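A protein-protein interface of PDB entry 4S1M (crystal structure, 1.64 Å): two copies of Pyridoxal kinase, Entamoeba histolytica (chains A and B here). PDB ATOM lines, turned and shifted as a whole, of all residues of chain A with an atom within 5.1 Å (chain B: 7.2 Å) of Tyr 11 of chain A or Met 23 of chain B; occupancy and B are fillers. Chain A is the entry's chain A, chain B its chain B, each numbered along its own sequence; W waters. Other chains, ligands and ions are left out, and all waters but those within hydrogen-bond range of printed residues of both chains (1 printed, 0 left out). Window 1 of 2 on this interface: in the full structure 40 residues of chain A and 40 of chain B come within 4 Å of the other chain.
Tyr 11 of chain A touches Met 23 of chain B, but with the chains exchanged Met 23 of chain A does not touch Tyr 11 of chain B (4.3 Å).
Arg 20 of chain A touches Met 23 of chain B, and with the chains exchanged Met 23 of chain A touches Arg 20 of chain B.
Leu 37 of chain A touches its own counterpart, Leu 37 of chain B.
Of the 15 pairs that touch across the chains among the printed residues, 6 have their exchanged pair printed and touching as well.
Hydrophobic or aromatic side chains of chain A that line the printed part of chain B: Tyr 11, Met 23, Leu 37 and His 40.
Printed residues of chain B that touch a printed residue of chain A: Tyr 11, Arg 20, Met 23, Asp 27, Ile 34, Phe 35, Val 36, Leu 37 and Ile 63.
Hydrophobic or aromatic side chains of chain B within 4 Å of the printed part of chain A: Tyr 11, Met 23, Ile 34, Phe 35, Leu 37 and Ile 63.
Among the printed residues, 15 pairs touch across the chains.
Among the printed residues, Asp or Glu carboxylates within 4 Å of a Lys or Arg side-chain nitrogen of the other chain: Arg 20 of chain A with Asp 27 of chain B.
CE of Met 23 of chain B touches OH of Tyr 11 of chain A (3.1 Å).
Tyr 11 of chain A touches Leu 37 of chain B (OH to CD2, 3.6 Å).
Cys 13 of chain A touches Ile 34 of chain B.
Val 36 of chain B touches Cys 13 of chain A (CA to SG, 3.8 Å).
Arg 20 of chain A touches Phe 35 of chain B.
CE of Met 23 of chain A touches NH1 of Arg 20 of chain B, at 3.2 Å.
Tyr 11 of chain B touches Leu 37 of chain A (OH to CD2, 3.6 Å).
CD1 of Leu 37 of chain A touches CD1 of Leu 37 of chain B (3.6 Å).
Ile 63 of chain B touches His 40 of chain A.
NE2 of His 40 of chain A is in hydrogen-bond range of N of Leu 37 of chain B, 3.2 Å away.
The backbone carbonyl oxygen (O) of Cys 13 of chain A lies within hydrogen-bond range of the backbone NH (N) of Phe 35 of chain B (2.9 Å).
The side-chain sulfur (SD) of Met 23 of chain A sits close to the side-chain sulfur (SD) of Met 23 of chain B (3.7 Å).
OH of Tyr 11 of chain A lies within hydrogen-bond range of O of Phe 35 of chain B, 2.7 Å away.
The guanidinium group (NH2) of Arg 20 of chain A lies within salt-bridge range of the side-chain carboxylate (OD1) of Asp 27 of chain B, 2.8 Å away.
The backbone carbonyl oxygen of Leu 41 of chain A lies within hydrogen-bond range of the backbone NH of Cys 13 of chain A.
The backbone NH of Thr 7 of chain B lies within hydrogen-bond range of the backbone carbonyl oxygen of Ile 34 of chain B (2.9 Å).
The backbone NH (N) of Tyr 11 of chain A lies within hydrogen-bond range of the side-chain hydroxyl (OG1) of Thr 39 of chain A (2.9 Å).
The backbone NH (N) of Leu 41 of chain A lies within hydrogen-bond range of the backbone carbonyl oxygen (O) of Tyr 11 of chain A (3.1 Å).
Tyr 11 of chain A touches just these residues of chain B: Met 23 (3.1 Å), Phe 35 (2.7 Å) and Leu 37 (3.6 Å).
Of the printed residues of chain B, Arg 20 of chain A touches Met 23, Asp 27 and Phe 35.
Of the printed residues of chain A, Met 23 of chain B touches Tyr 11, Arg 20 and Met 23.
Of the printed residues of chain A, Ile 34 of chain B touches Cys 13.
The nearest residue of chain B that does not touch Tyr 11 of chain A is Val 36 of chain B (4.9 Å).
The nearest printed residue of chain A that does not touch Met 23 of chain B is Val 12 of chain A (6.7 Å).
The nearest printed residue of chain B that does not touch Cys 13 of chain A is Ile 63 of chain B (4.02 Å).
Water W1 lies within hydrogen-bond range of O of Ser 33 of chain B (2.6 Å) and NH2 of Arg 20 of chain A (3.1 Å).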
ATOM      1  N   SER A   9      -3.848  16.641 -29.349  1.00  0.00           N
ATOM      2  CA  SER A   9      -4.876  17.474 -28.808  1.00  0.00           C
ATOM      3  C   SER A   9      -5.700  16.756 -27.725  1.00  0.00           C
ATOM      4  O   SER A   9      -5.354  15.645 -27.353  1.00  0.00           O
ATOM      5  CB  SER A   9      -5.800  17.964 -29.959  1.00  0.00           C
ATOM      6  OG  SER A   9      -6.582  19.074 -29.493  1.00  0.00           O
ATOM      7  N   SER A  10      -6.717  17.431 -27.233  1.00  0.00           N
ATOM      8  CA  SER A  10      -7.517  16.960 -26.083  1.00  0.00           C
ATOM      9  C   SER A  10      -8.418  15.826 -26.464  1.00  0.00           C
ATOM     10  O   SER A  10      -8.673  15.517 -27.610  1.00  0.00           O
ATOM     11  CB  SER A  10      -8.399  18.094 -25.545  1.00  0.00           C
ATOM     12  OG  SER A  10      -9.107  18.668 -26.651  1.00  0.00           O
ATOM     13  N   TYR A  11      -8.862  15.126 -25.411  1.00  0.00           N
ATOM     14  CA  TYR A  11      -9.796  14.006 -25.547  1.00  0.00           C
ATOM     15  C   TYR A  11     -10.875  14.093 -24.476  1.00  0.00           C
ATOM     16  O   TYR A  11     -10.596  14.334 -23.280  1.00  0.00           O
ATOM     17  CB  TYR A  11      -9.045  12.668 -25.404  1.00  0.00           C
ATOM     18  CG  TYR A  11      -9.975  11.484 -25.507  1.00  0.00           C
ATOM     19  CD1 TYR A  11     -10.298  10.976 -26.714  1.00  0.00           C
ATOM     20  CD2 TYR A  11     -10.469  10.882 -24.379  1.00  0.00           C
ATOM     21  CE1 TYR A  11     -11.192   9.916 -26.848  1.00  0.00           C
ATOM     22  CE2 TYR A  11     -11.383   9.858 -24.439  1.00  0.00           C
ATOM     23  CZ  TYR A  11     -11.711   9.322 -25.691  1.00  0.00           C
ATOM     24  OH  TYR A  11     -12.654   8.302 -25.817  1.00  0.00           O
ATOM     25  N   VAL A  12     -12.100  13.835 -24.890  1.00  0.00           N
ATOM     26  CA  VAL A  12     -13.220  13.727 -24.013  1.00  0.00           C
ATOM     27  C   VAL A  12     -13.931  12.403 -24.251  1.00  0.00           C
ATOM     28  O   VAL A  12     -14.061  11.974 -25.447  1.00  0.00           O
ATOM     29  CB  VAL A  12     -14.237  14.898 -24.179  1.00  0.00           C
ATOM     30  CG1 VAL A  12     -13.659  16.147 -23.629  1.00  0.00           C
ATOM     31  CG2 VAL A  12     -14.667  15.057 -25.611  1.00  0.00           C
ATOM     32  N   CYS A  13     -14.381  11.746 -23.191  1.00  0.00           N
ATOM     33  CA  CYS A  13     -15.029  10.407 -23.285  1.00  0.00           C
ATOM     34  C   CYS A  13     -16.396  10.491 -23.879  1.00  0.00           C
ATOM     35  O   CYS A  13     -16.810   9.601 -24.618  1.00  0.00           O
ATOM     36  CB  CYS A  13     -15.113   9.737 -21.944  1.00  0.00           C
ATOM     37  SG  CYS A  13     -13.507   9.439 -21.150  1.00  0.00           S
ATOM     38  N   ASN A  19      -9.116  16.134 -30.243  1.00  0.00           N
ATOM     39  CA  ASN A  19      -8.854  14.945 -30.972  1.00  0.00           C
ATOM     40  C   ASN A  19      -9.979  13.998 -31.181  1.00  0.00           C
ATOM     41  O   ASN A  19      -9.905  13.151 -32.076  1.00  0.00           O
ATOM     42  CB  ASN A  19      -7.637  14.176 -30.361  1.00  0.00           C
ATOM     43  CG  ASN A  19      -6.329  14.394 -31.145  1.00  0.00           C
ATOM     44  OD1 ASN A  19      -6.280  14.922 -32.214  1.00  0.00           O
ATOM     45  ND2 ASN A  19      -5.249  13.894 -30.562  1.00  0.00           N
ATOM     46  N   ARG A  20     -11.039  14.084 -30.396  1.00  0.00           N
ATOM     47  CA  ARG A  20     -12.207  13.309 -30.724  1.00  0.00           C
ATOM     48  C   ARG A  20     -12.867  13.780 -31.983  1.00  0.00           C
ATOM     49  O   ARG A  20     -13.276  12.978 -32.814  1.00  0.00           O
ATOM     50  CB  ARG A  20     -13.144  13.319 -29.509  1.00  0.00           C
ATOM     51  CG  ARG A  20     -14.298  12.470 -29.698  1.00  0.00           C
ATOM     52  CD  ARG A  20     -13.921  10.924 -29.626  1.00  0.00           C
ATOM     53  NE  ARG A  20     -15.152  10.255 -29.788  1.00  0.00           N
ATOM     54  CZ  ARG A  20     -15.562   9.597 -30.852  1.00  0.00           C
ATOM     55  NH1 ARG A  20     -14.694   9.144 -31.769  1.00  0.00           N
ATOM     56  NH2 ARG A  20     -16.794   9.193 -30.882  1.00  0.00           N
ATOM     57  N   MET A  23     -10.562  12.535 -34.710  1.00  0.00           N
ATOM     58  CA  MET A  23     -10.787  11.126 -35.001  1.00  0.00           C
ATOM     59  C   MET A  23     -11.990  10.916 -35.917  1.00  0.00           C
ATOM     60  O   MET A  23     -11.890  10.215 -36.924  1.00  0.00           O
ATOM     61  CB  MET A  23     -10.971  10.335 -33.704  1.00  0.00           C
ATOM     62  CG  MET A  23      -9.813  10.464 -32.728  1.00  0.00           C
ATOM     63  SD  MET A  23     -10.025   9.439 -31.259  1.00  0.00           S
ATOM     64  CE  MET A  23     -11.226   8.249 -31.847  1.00  0.00           C
ATOM     65  N   LEU A  37      -3.120  11.986 -27.197  1.00  0.00           N
ATOM     66  CA  LEU A  37      -4.003  12.745 -26.331  1.00  0.00           C
ATOM     67  C   LEU A  37      -3.255  13.620 -25.395  1.00  0.00           C
ATOM     68  O   LEU A  37      -2.189  13.261 -24.867  1.00  0.00           O
ATOM     69  CB  LEU A  37      -4.971  11.795 -25.586  1.00  0.00           C
ATOM     70  CG  LEU A  37      -5.630  10.703 -26.432  1.00  0.00           C
ATOM     71  CD1 LEU A  37      -6.578   9.932 -25.567  1.00  0.00           C
ATOM     72  CD2 LEU A  37      -6.254  11.269 -27.690  1.00  0.00           C
ATOM     73  N   THR A  38      -3.844  14.803 -25.104  1.00  0.00           N
ATOM     74  CA  THR A  38      -3.260  15.712 -24.120  1.00  0.00           C
ATOM     75  C   THR A  38      -4.078  15.795 -22.817  1.00  0.00           C
ATOM     76  O   THR A  38      -3.657  16.374 -21.839  1.00  0.00           O
ATOM     77  CB  THR A  38      -3.068  17.123 -24.691  1.00  0.00           C
ATOM     78  OG1 THR A  38      -4.373  17.642 -24.969  1.00  0.00           O
ATOM     79  CG2 THR A  38      -2.185  17.130 -25.896  1.00  0.00           C
ATOM     80  N   THR A  39      -5.300  15.187 -22.819  1.00  0.00           N
ATOM     81  CA  THR A  39      -6.185  15.086 -21.695  1.00  0.00           C
ATOM     82  C   THR A  39      -6.961  13.781 -21.822  1.00  0.00           C
ATOM     83  O   THR A  39      -7.035  13.217 -22.910  1.00  0.00           O
ATOM     84  CB  THR A  39      -7.268  16.227 -21.645  1.00  0.00           C
ATOM     85  OG1 THR A  39      -8.209  16.056 -22.718  1.00  0.00           O
ATOM     86  CG2 THR A  39      -6.637  17.531 -21.785  1.00  0.00           C
ATOM     87  N   HIS A  40      -7.496  13.348 -20.700  1.00  0.00           N
ATOM     88  CA  HIS A  40      -8.486  12.280 -20.665  1.00  0.00           C
ATOM     89  C   HIS A  40      -9.577  12.723 -19.742  1.00  0.00           C
ATOM     90  O   HIS A  40      -9.575  12.484 -18.525  1.00  0.00           O
ATOM     91  CB  HIS A  40      -7.825  10.990 -20.209  1.00  0.00           C
ATOM     92  CG  HIS A  40      -8.741   9.814 -20.159  1.00  0.00           C
ATOM     93  ND1 HIS A  40      -8.538   8.763 -19.296  1.00  0.00           N
ATOM     94  CD2 HIS A  40      -9.880   9.532 -20.832  1.00  0.00           C
ATOM     95  CE1 HIS A  40      -9.510   7.881 -19.450  1.00  0.00           C
ATOM     96  NE2 HIS A  40     -10.314   8.306 -20.399  1.00  0.00           N
ATOM     97  N   LEU A  41     -10.505  13.482 -20.302  1.00  0.00           N
ATOM     98  CA  LEU A  41     -11.587  14.054 -19.531  1.00  0.00           C
ATOM     99  C   LEU A  41     -12.901  13.374 -19.845  1.00  0.00           C
ATOM    100  O   LEU A  41     -13.103  12.855 -20.950  1.00  0.00           O
ATOM    101  CB  LEU A  41     -11.757  15.557 -19.903  1.00  0.00           C
ATOM    102  CG  LEU A  41     -10.490  16.377 -19.783  1.00  0.00           C
ATOM    103  CD1 LEU A  41     -10.834  17.768 -20.287  1.00  0.00           C
ATOM    104  CD2 LEU A  41     -10.012  16.453 -18.350  1.00  0.00           C
ATOM    105  N   THR B   7     -18.680   2.345 -23.264  1.00  0.00           N
ATOM    106  CA  THR B   7     -17.650   1.304 -23.474  1.00  0.00           C
ATOM    107  C   THR B   7     -16.350   1.691 -22.774  1.00  0.00           C
ATOM    108  O   THR B   7     -15.843   2.808 -22.934  1.00  0.00           O
ATOM    109  CB  THR B   7     -17.449   0.978 -24.941  1.00  0.00           C
ATOM    110  OG1 THR B   7     -16.244   0.197 -25.144  1.00  0.00           O
ATOM    111  CG2 THR B   7     -17.410   2.175 -25.854  1.00  0.00           C
ATOM    112  N   SER B   9     -12.568   0.481 -22.185  1.00  0.00           N
ATOM    113  CA  SER B   9     -11.519  -0.391 -22.724  1.00  0.00           C
ATOM    114  C   SER B   9     -10.276   0.417 -23.091  1.00  0.00           C
ATOM    115  O   SER B   9     -10.180   1.614 -22.808  1.00  0.00           O
ATOM    116  CB  SER B   9     -12.017  -1.132 -24.011  1.00  0.00           C
ATOM    117  OG  SER B   9     -11.140  -2.248 -24.313  1.00  0.00           O
ATOM    118  N   SER B  10      -9.312  -0.252 -23.699  1.00  0.00           N
ATOM    119  CA  SER B  10      -7.973   0.304 -23.929  1.00  0.00           C
ATOM    120  C   SER B  10      -7.935   1.301 -25.068  1.00  0.00           C
ATOM    121  O   SER B  10      -8.873   1.398 -25.879  1.00  0.00           O
ATOM    122  CB  SER B  10      -6.981  -0.828 -24.225  1.00  0.00           C
ATOM    123  OG  SER B  10      -7.504  -1.618 -25.262  1.00  0.00           O
ATOM    124  N   TYR B  11      -6.855   2.068 -25.106  1.00  0.00           N
ATOM    125  CA  TYR B  11      -6.626   3.056 -26.179  1.00  0.00           C
ATOM    126  C   TYR B  11      -5.220   3.036 -26.639  1.00  0.00           C
ATOM    127  O   TYR B  11      -4.289   3.040 -25.798  1.00  0.00           O
ATOM    128  CB  TYR B  11      -7.053   4.455 -25.703  1.00  0.00           C
ATOM    129  CG  TYR B  11      -6.822   5.551 -26.750  1.00  0.00           C
ATOM    130  CD1 TYR B  11      -7.765   5.826 -27.700  1.00  0.00           C
ATOM    131  CD2 TYR B  11      -5.628   6.205 -26.837  1.00  0.00           C
ATOM    132  CE1 TYR B  11      -7.557   6.721 -28.731  1.00  0.00           C
ATOM    133  CE2 TYR B  11      -5.406   7.187 -27.803  1.00  0.00           C
ATOM    134  CZ  TYR B  11      -6.378   7.450 -28.780  1.00  0.00           C
ATOM    135  OH  TYR B  11      -6.163   8.377 -29.758  1.00  0.00           O
ATOM    136  N   VAL B  17      -6.861  -1.187 -31.533  1.00  0.00           N
ATOM    137  CA  VAL B  17      -7.302  -2.150 -30.520  1.00  0.00           C
ATOM    138  C   VAL B  17      -8.301  -1.477 -29.605  1.00  0.00           C
ATOM    139  O   VAL B  17      -8.422  -0.221 -29.626  1.00  0.00           O
ATOM    140  CB  VAL B  17      -6.154  -2.739 -29.637  1.00  0.00           C
ATOM    141  CG1 VAL B  17      -5.097  -3.405 -30.496  1.00  0.00           C
ATOM    142  CG2 VAL B  17      -5.615  -1.681 -28.720  1.00  0.00           C
ATOM    143  N   GLY B  18      -9.015  -2.274 -28.842  1.00  0.00           N
ATOM    144  CA  GLY B  18      -9.861  -1.835 -27.767  1.00  0.00           C
ATOM    145  C   GLY B  18     -10.840  -0.736 -28.100  1.00  0.00           C
ATOM    146  O   GLY B  18     -11.564  -0.813 -29.124  1.00  0.00           O
ATOM    147  N   ASN B  19     -10.867   0.291 -27.253  1.00  0.00           N
ATOM    148  CA  ASN B  19     -11.791   1.429 -27.560  1.00  0.00           C
ATOM    149  C   ASN B  19     -11.517   2.167 -28.836  1.00  0.00           C
ATOM    150  O   ASN B  19     -12.405   2.885 -29.337  1.00  0.00           O
ATOM    151  CB  ASN B  19     -11.868   2.377 -26.363  1.00  0.00           C
ATOM    152  CG  ASN B  19     -13.127   2.181 -25.533  1.00  0.00           C
ATOM    153  OD1 ASN B  19     -14.090   1.473 -25.931  1.00  0.00           O
ATOM    154  ND2 ASN B  19     -13.169   2.816 -24.382  1.00  0.00           N
ATOM    155  N   ARG B  20     -10.304   2.162 -29.366  1.00  0.00           N
ATOM    156  CA  ARG B  20     -10.060   2.732 -30.645  1.00  0.00           C
ATOM    157  C   ARG B  20     -10.799   2.018 -31.813  1.00  0.00           C
ATOM    158  O   ARG B  20     -11.407   2.642 -32.699  1.00  0.00           O
ATOM    159  CB  ARG B  20      -8.585   2.851 -30.948  1.00  0.00           C
ATOM    160  CG  ARG B  20      -8.275   3.557 -32.234  1.00  0.00           C
ATOM    161  CD  ARG B  20      -8.580   5.077 -32.224  1.00  0.00           C
ATOM    162  NE  ARG B  20      -8.198   5.537 -33.546  1.00  0.00           N
ATOM    163  CZ  ARG B  20      -8.990   6.083 -34.480  1.00  0.00           C
ATOM    164  NH1 ARG B  20     -10.282   6.317 -34.263  1.00  0.00           N
ATOM    165  NH2 ARG B  20      -8.509   6.265 -35.662  1.00  0.00           N
ATOM    166  N   CYS B  21     -10.788   0.686 -31.767  1.00  0.00           N
ATOM    167  CA  CYS B  21     -11.705  -0.116 -32.642  1.00  0.00           C
ATOM    168  C   CYS B  21     -13.155   0.255 -32.363  1.00  0.00           C
ATOM    169  O   CYS B  21     -13.948   0.482 -33.330  1.00  0.00           O
ATOM    170  CB  CYS B  21     -11.589  -1.615 -32.422  1.00  0.00           C
ATOM    171  SG  CYS B  21      -9.984  -2.222 -32.880  1.00  0.00           S
ATOM    172  N   GLY B  22     -13.493   0.328 -31.086  1.00  0.00           N
ATOM    173  CA  GLY B  22     -14.842   0.734 -30.658  1.00  0.00           C
ATOM    174  C   GLY B  22     -15.259   2.072 -31.300  1.00  0.00           C
ATOM    175  O   GLY B  22     -16.395   2.197 -31.842  1.00  0.00           O
ATOM    176  N   MET B  23     -14.393   3.052 -31.268  1.00  0.00           N
ATOM    177  CA  MET B  23     -14.745   4.347 -31.823  1.00  0.00           C
ATOM    178  C   MET B  23     -15.003   4.242 -33.323  1.00  0.00           C
ATOM    179  O   MET B  23     -16.007   4.730 -33.833  1.00  0.00           O
ATOM    180  CB  MET B  23     -13.629   5.349 -31.545  1.00  0.00           C
ATOM    181  CG  MET B  23     -13.405   5.687 -30.067  1.00  0.00           C
ATOM    182  SD  MET B  23     -11.778   6.554 -29.684  1.00  0.00           S
ATOM    183  CE  MET B  23     -11.679   6.283 -27.957  1.00  0.00           C
ATOM    184  N   ILE B  24     -14.103   3.706 -34.068  1.00  0.00           N
ATOM    185  CA  ILE B  24     -14.209   3.628 -35.538  1.00  0.00           C
ATOM    186  C   ILE B  24     -15.487   2.909 -35.946  1.00  0.00           C
ATOM    187  O   ILE B  24     -16.236   3.374 -36.833  1.00  0.00           O
ATOM    188  CB  ILE B  24     -13.025   2.875 -36.163  1.00  0.00           C
ATOM    189  CG1 ILE B  24     -11.817   3.721 -35.905  1.00  0.00           C
ATOM    190  CG2 ILE B  24     -13.235   2.720 -37.688  1.00  0.00           C
ATOM    191  CD1 ILE B  24     -10.524   2.965 -36.237  1.00  0.00           C
ATOM    192  N   ILE B  25     -15.768   1.802 -35.262  1.00  0.00           N
ATOM    193  CA  ILE B  25     -16.933   1.032 -35.599  1.00  0.00           C
ATOM    194  C   ILE B  25     -18.267   1.695 -35.154  1.00  0.00           C
ATOM    195  O   ILE B  25     -19.154   1.907 -35.997  1.00  0.00           O
ATOM    196  CB  ILE B  25     -16.835  -0.367 -35.030  1.00  0.00           C
ATOM    197  CG1 ILE B  25     -15.648  -1.044 -35.738  1.00  0.00           C
ATOM    198  CG2 ILE B  25     -18.162  -1.144 -35.239  1.00  0.00           C
ATOM    199  CD1 ILE B  25     -15.096  -2.209 -34.945  1.00  0.00           C
ATOM    200  N   LEU B  26     -18.342   2.104 -33.901  1.00  0.00           N
ATOM    201  CA  LEU B  26     -19.565   2.737 -33.403  1.00  0.00           C
ATOM    202  C   LEU B  26     -19.794   4.085 -34.110  1.00  0.00           C
ATOM    203  O   LEU B  26     -20.944   4.380 -34.450  1.00  0.00           O
ATOM    204  CB  LEU B  26     -19.569   2.863 -31.891  1.00  0.00           C
ATOM    205  CG  LEU B  26     -19.662   1.526 -31.147  1.00  0.00           C
ATOM    206  CD1 LEU B  26     -19.323   1.686 -29.706  1.00  0.00           C
ATOM    207  CD2 LEU B  26     -21.071   0.979 -31.259  1.00  0.00           C
ATOM    208  N   ASP B  27     -18.751   4.852 -34.336  1.00  0.00           N
ATOM    209  CA  ASP B  27     -18.898   6.096 -35.127  1.00  0.00           C
ATOM    210  C   ASP B  27     -19.465   5.801 -36.520  1.00  0.00           C
ATOM    211  O   ASP B  27     -20.380   6.464 -37.012  1.00  0.00           O
ATOM    212  CB  ASP B  27     -17.563   6.805 -35.293  1.00  0.00           C
ATOM    213  CG  ASP B  27     -17.035   7.458 -34.009  1.00  0.00           C
ATOM    214  OD1 ASP B  27     -17.714   7.524 -32.960  1.00  0.00           O
ATOM    215  OD2 ASP B  27     -15.826   7.878 -34.041  1.00  0.00           O
ATOM    216  N   SER B  28     -18.944   4.752 -37.191  1.00  0.00           N
ATOM    217  CA  SER B  28     -19.354   4.458 -38.570  1.00  0.00           C
ATOM    218  C   SER B  28     -20.824   3.971 -38.624  1.00  0.00           C
ATOM    219  O   SER B  28     -21.528   4.220 -39.591  1.00  0.00           O
ATOM    220  CB  SER B  28     -18.449   3.392 -39.167  1.00  0.00           C
ATOM    221  OG  SER B  28     -17.137   3.956 -39.230  1.00  0.00           O
ATOM    222  N   PHE B  29     -21.281   3.357 -37.546  1.00  0.00           N
ATOM    223  CA  PHE B  29     -22.704   2.988 -37.375  1.00  0.00           C
ATOM    224  C   PHE B  29     -23.569   4.142 -36.828  1.00  0.00           C
ATOM    225  O   PHE B  29     -24.816   3.980 -36.703  1.00  0.00           O
ATOM    226  CB  PHE B  29     -22.834   1.782 -36.456  1.00  0.00           C
ATOM    227  CG  PHE B  29     -22.695   0.404 -37.141  1.00  0.00           C
ATOM    228  CD1 PHE B  29     -21.465  -0.213 -37.300  1.00  0.00           C
ATOM    229  CD2 PHE B  29     -23.819  -0.308 -37.560  1.00  0.00           C
ATOM    230  CE1 PHE B  29     -21.343  -1.455 -37.884  1.00  0.00           C
ATOM    231  CE2 PHE B  29     -23.711  -1.577 -38.120  1.00  0.00           C
ATOM    232  CZ  PHE B  29     -22.471  -2.155 -38.295  1.00  0.00           C
ATOM    233  N   ILE B  31     -23.762   5.321 -33.880  1.00  0.00           N
ATOM    234  CA  ILE B  31     -24.235   5.003 -32.555  1.00  0.00           C
ATOM    235  C   ILE B  31     -23.506   5.875 -31.535  1.00  0.00           C
ATOM    236  O   ILE B  31     -22.283   5.758 -31.341  1.00  0.00           O
ATOM    237  CB  ILE B  31     -24.071   3.504 -32.222  1.00  0.00           C
ATOM    238  CG1 ILE B  31     -24.855   2.624 -33.219  1.00  0.00           C
ATOM    239  CG2 ILE B  31     -24.519   3.212 -30.800  1.00  0.00           C
ATOM    240  CD1 ILE B  31     -24.512   1.151 -33.204  1.00  0.00           C
ATOM    241  N   SER B  33     -21.911   7.156 -28.369  1.00  0.00           N
ATOM    242  CA  SER B  33     -21.284   6.366 -27.365  1.00  0.00           C
ATOM    243  C   SER B  33     -20.328   7.151 -26.497  1.00  0.00           C
ATOM    244  O   SER B  33     -19.743   8.135 -26.983  1.00  0.00           O
ATOM    245  CB  SER B  33     -20.523   5.230 -28.052  1.00  0.00           C
ATOM    246  OG  SER B  33     -21.396   4.469 -28.864  1.00  0.00           O
ATOM    247  N   ILE B  34     -20.132   6.696 -25.281  1.00  0.00           N
ATOM    248  CA  ILE B  34     -19.127   7.203 -24.391  1.00  0.00           C
ATOM    249  C   ILE B  34     -17.923   6.233 -24.374  1.00  0.00           C
ATOM    250  O   ILE B  34     -18.134   5.040 -24.136  1.00  0.00           O
ATOM    251  CB  ILE B  34     -19.643   7.292 -22.948  1.00  0.00           C
ATOM    252  CG1 ILE B  34     -20.905   8.157 -22.870  1.00  0.00           C
ATOM    253  CG2 ILE B  34     -18.522   7.830 -22.059  1.00  0.00           C
ATOM    254  CD1 ILE B  34     -21.617   8.044 -21.530  1.00  0.00           C
ATOM    255  N   PHE B  35     -16.710   6.743 -24.600  1.00  0.00           N
ATOM    256  CA  PHE B  35     -15.534   5.919 -24.648  1.00  0.00           C
ATOM    257  C   PHE B  35     -14.653   6.301 -23.485  1.00  0.00           C
ATOM    258  O   PHE B  35     -13.846   7.255 -23.576  1.00  0.00           O
ATOM    259  CB  PHE B  35     -14.802   6.096 -25.964  1.00  0.00           C
ATOM    260  CG  PHE B  35     -15.595   5.758 -27.166  1.00  0.00           C
ATOM    261  CD1 PHE B  35     -16.419   6.694 -27.836  1.00  0.00           C
ATOM    262  CD2 PHE B  35     -15.591   4.411 -27.613  1.00  0.00           C
ATOM    263  CE1 PHE B  35     -17.183   6.341 -28.948  1.00  0.00           C
ATOM    264  CE2 PHE B  35     -16.369   4.072 -28.738  1.00  0.00           C
ATOM    265  CZ  PHE B  35     -17.169   4.997 -29.364  1.00  0.00           C
ATOM    266  N   VAL B  36     -14.727   5.524 -22.389  1.00  0.00           N
ATOM    267  CA  VAL B  36     -13.852   5.703 -21.234  1.00  0.00           C
ATOM    268  C   VAL B  36     -12.623   4.854 -21.464  1.00  0.00           C
ATOM    269  O   VAL B  36     -12.720   3.660 -21.688  1.00  0.00           O
ATOM    270  CB  VAL B  36     -14.530   5.397 -19.897  1.00  0.00           C
ATOM    271  CG1 VAL B  36     -13.576   5.553 -18.724  1.00  0.00           C
ATOM    272  CG2 VAL B  36     -15.761   6.223 -19.721  1.00  0.00           C
ATOM    273  N   LEU B  37     -11.451   5.472 -21.375  1.00  0.00           N
ATOM    274  CA  LEU B  37     -10.218   4.738 -21.610  1.00  0.00           C
ATOM    275  C   LEU B  37      -9.649   4.123 -20.380  1.00  0.00           C
ATOM    276  O   LEU B  37      -9.728   4.662 -19.293  1.00  0.00           O
ATOM    277  CB  LEU B  37      -9.191   5.688 -22.268  1.00  0.00           C
ATOM    278  CG  LEU B  37      -9.689   6.588 -23.405  1.00  0.00           C
ATOM    279  CD1 LEU B  37      -8.554   7.365 -23.993  1.00  0.00           C
ATOM    280  CD2 LEU B  37     -10.459   5.759 -24.431  1.00  0.00           C
ATOM    281  N   ILE B  63     -13.687  10.530 -13.747  1.00  0.00           N
ATOM    282  CA  ILE B  63     -14.387  10.465 -15.029  1.00  0.00           C
ATOM    283  C   ILE B  63     -15.786   9.913 -14.905  1.00  0.00           C
ATOM    284  O   ILE B  63     -16.781  10.541 -15.340  1.00  0.00           O
ATOM    285  CB  ILE B  63     -13.598   9.692 -16.065  1.00  0.00           C
ATOM    286  CG1 ILE B  63     -12.389  10.511 -16.497  1.00  0.00           C
ATOM    287  CG2 ILE B  63     -14.457   9.351 -17.250  1.00  0.00           C
ATOM    288  CD1 ILE B  63     -11.354   9.706 -17.279  1.00  0.00           C
ATOM    289  N   TYR B 222     -17.294  -5.091 -31.422  1.00  0.00           N
ATOM    290  CA  TYR B 222     -18.054  -3.890 -31.729  1.00  0.00           C
ATOM    291  C   TYR B 222     -18.989  -4.001 -32.929  1.00  0.00           C
ATOM    292  O   TYR B 222     -20.032  -3.332 -32.968  1.00  0.00           O
ATOM    293  CB  TYR B 222     -17.134  -2.664 -31.816  1.00  0.00           C
ATOM    294  CG  TYR B 222     -16.573  -2.354 -30.443  1.00  0.00           C
ATOM    295  CD1 TYR B 222     -17.339  -1.727 -29.455  1.00  0.00           C
ATOM    296  CD2 TYR B 222     -15.259  -2.727 -30.082  1.00  0.00           C
ATOM    297  CE1 TYR B 222     -16.854  -1.518 -28.191  1.00  0.00           C
ATOM    298  CE2 TYR B 222     -14.777  -2.481 -28.810  1.00  0.00           C
ATOM    299  CZ  TYR B 222     -15.577  -1.890 -27.880  1.00  0.00           C
ATOM    300  OH  TYR B 222     -15.087  -1.687 -26.617  1.00  0.00           O
HETATM  301  O   HOH W   1     -18.278   9.854 -28.269  1.00  0.00           O
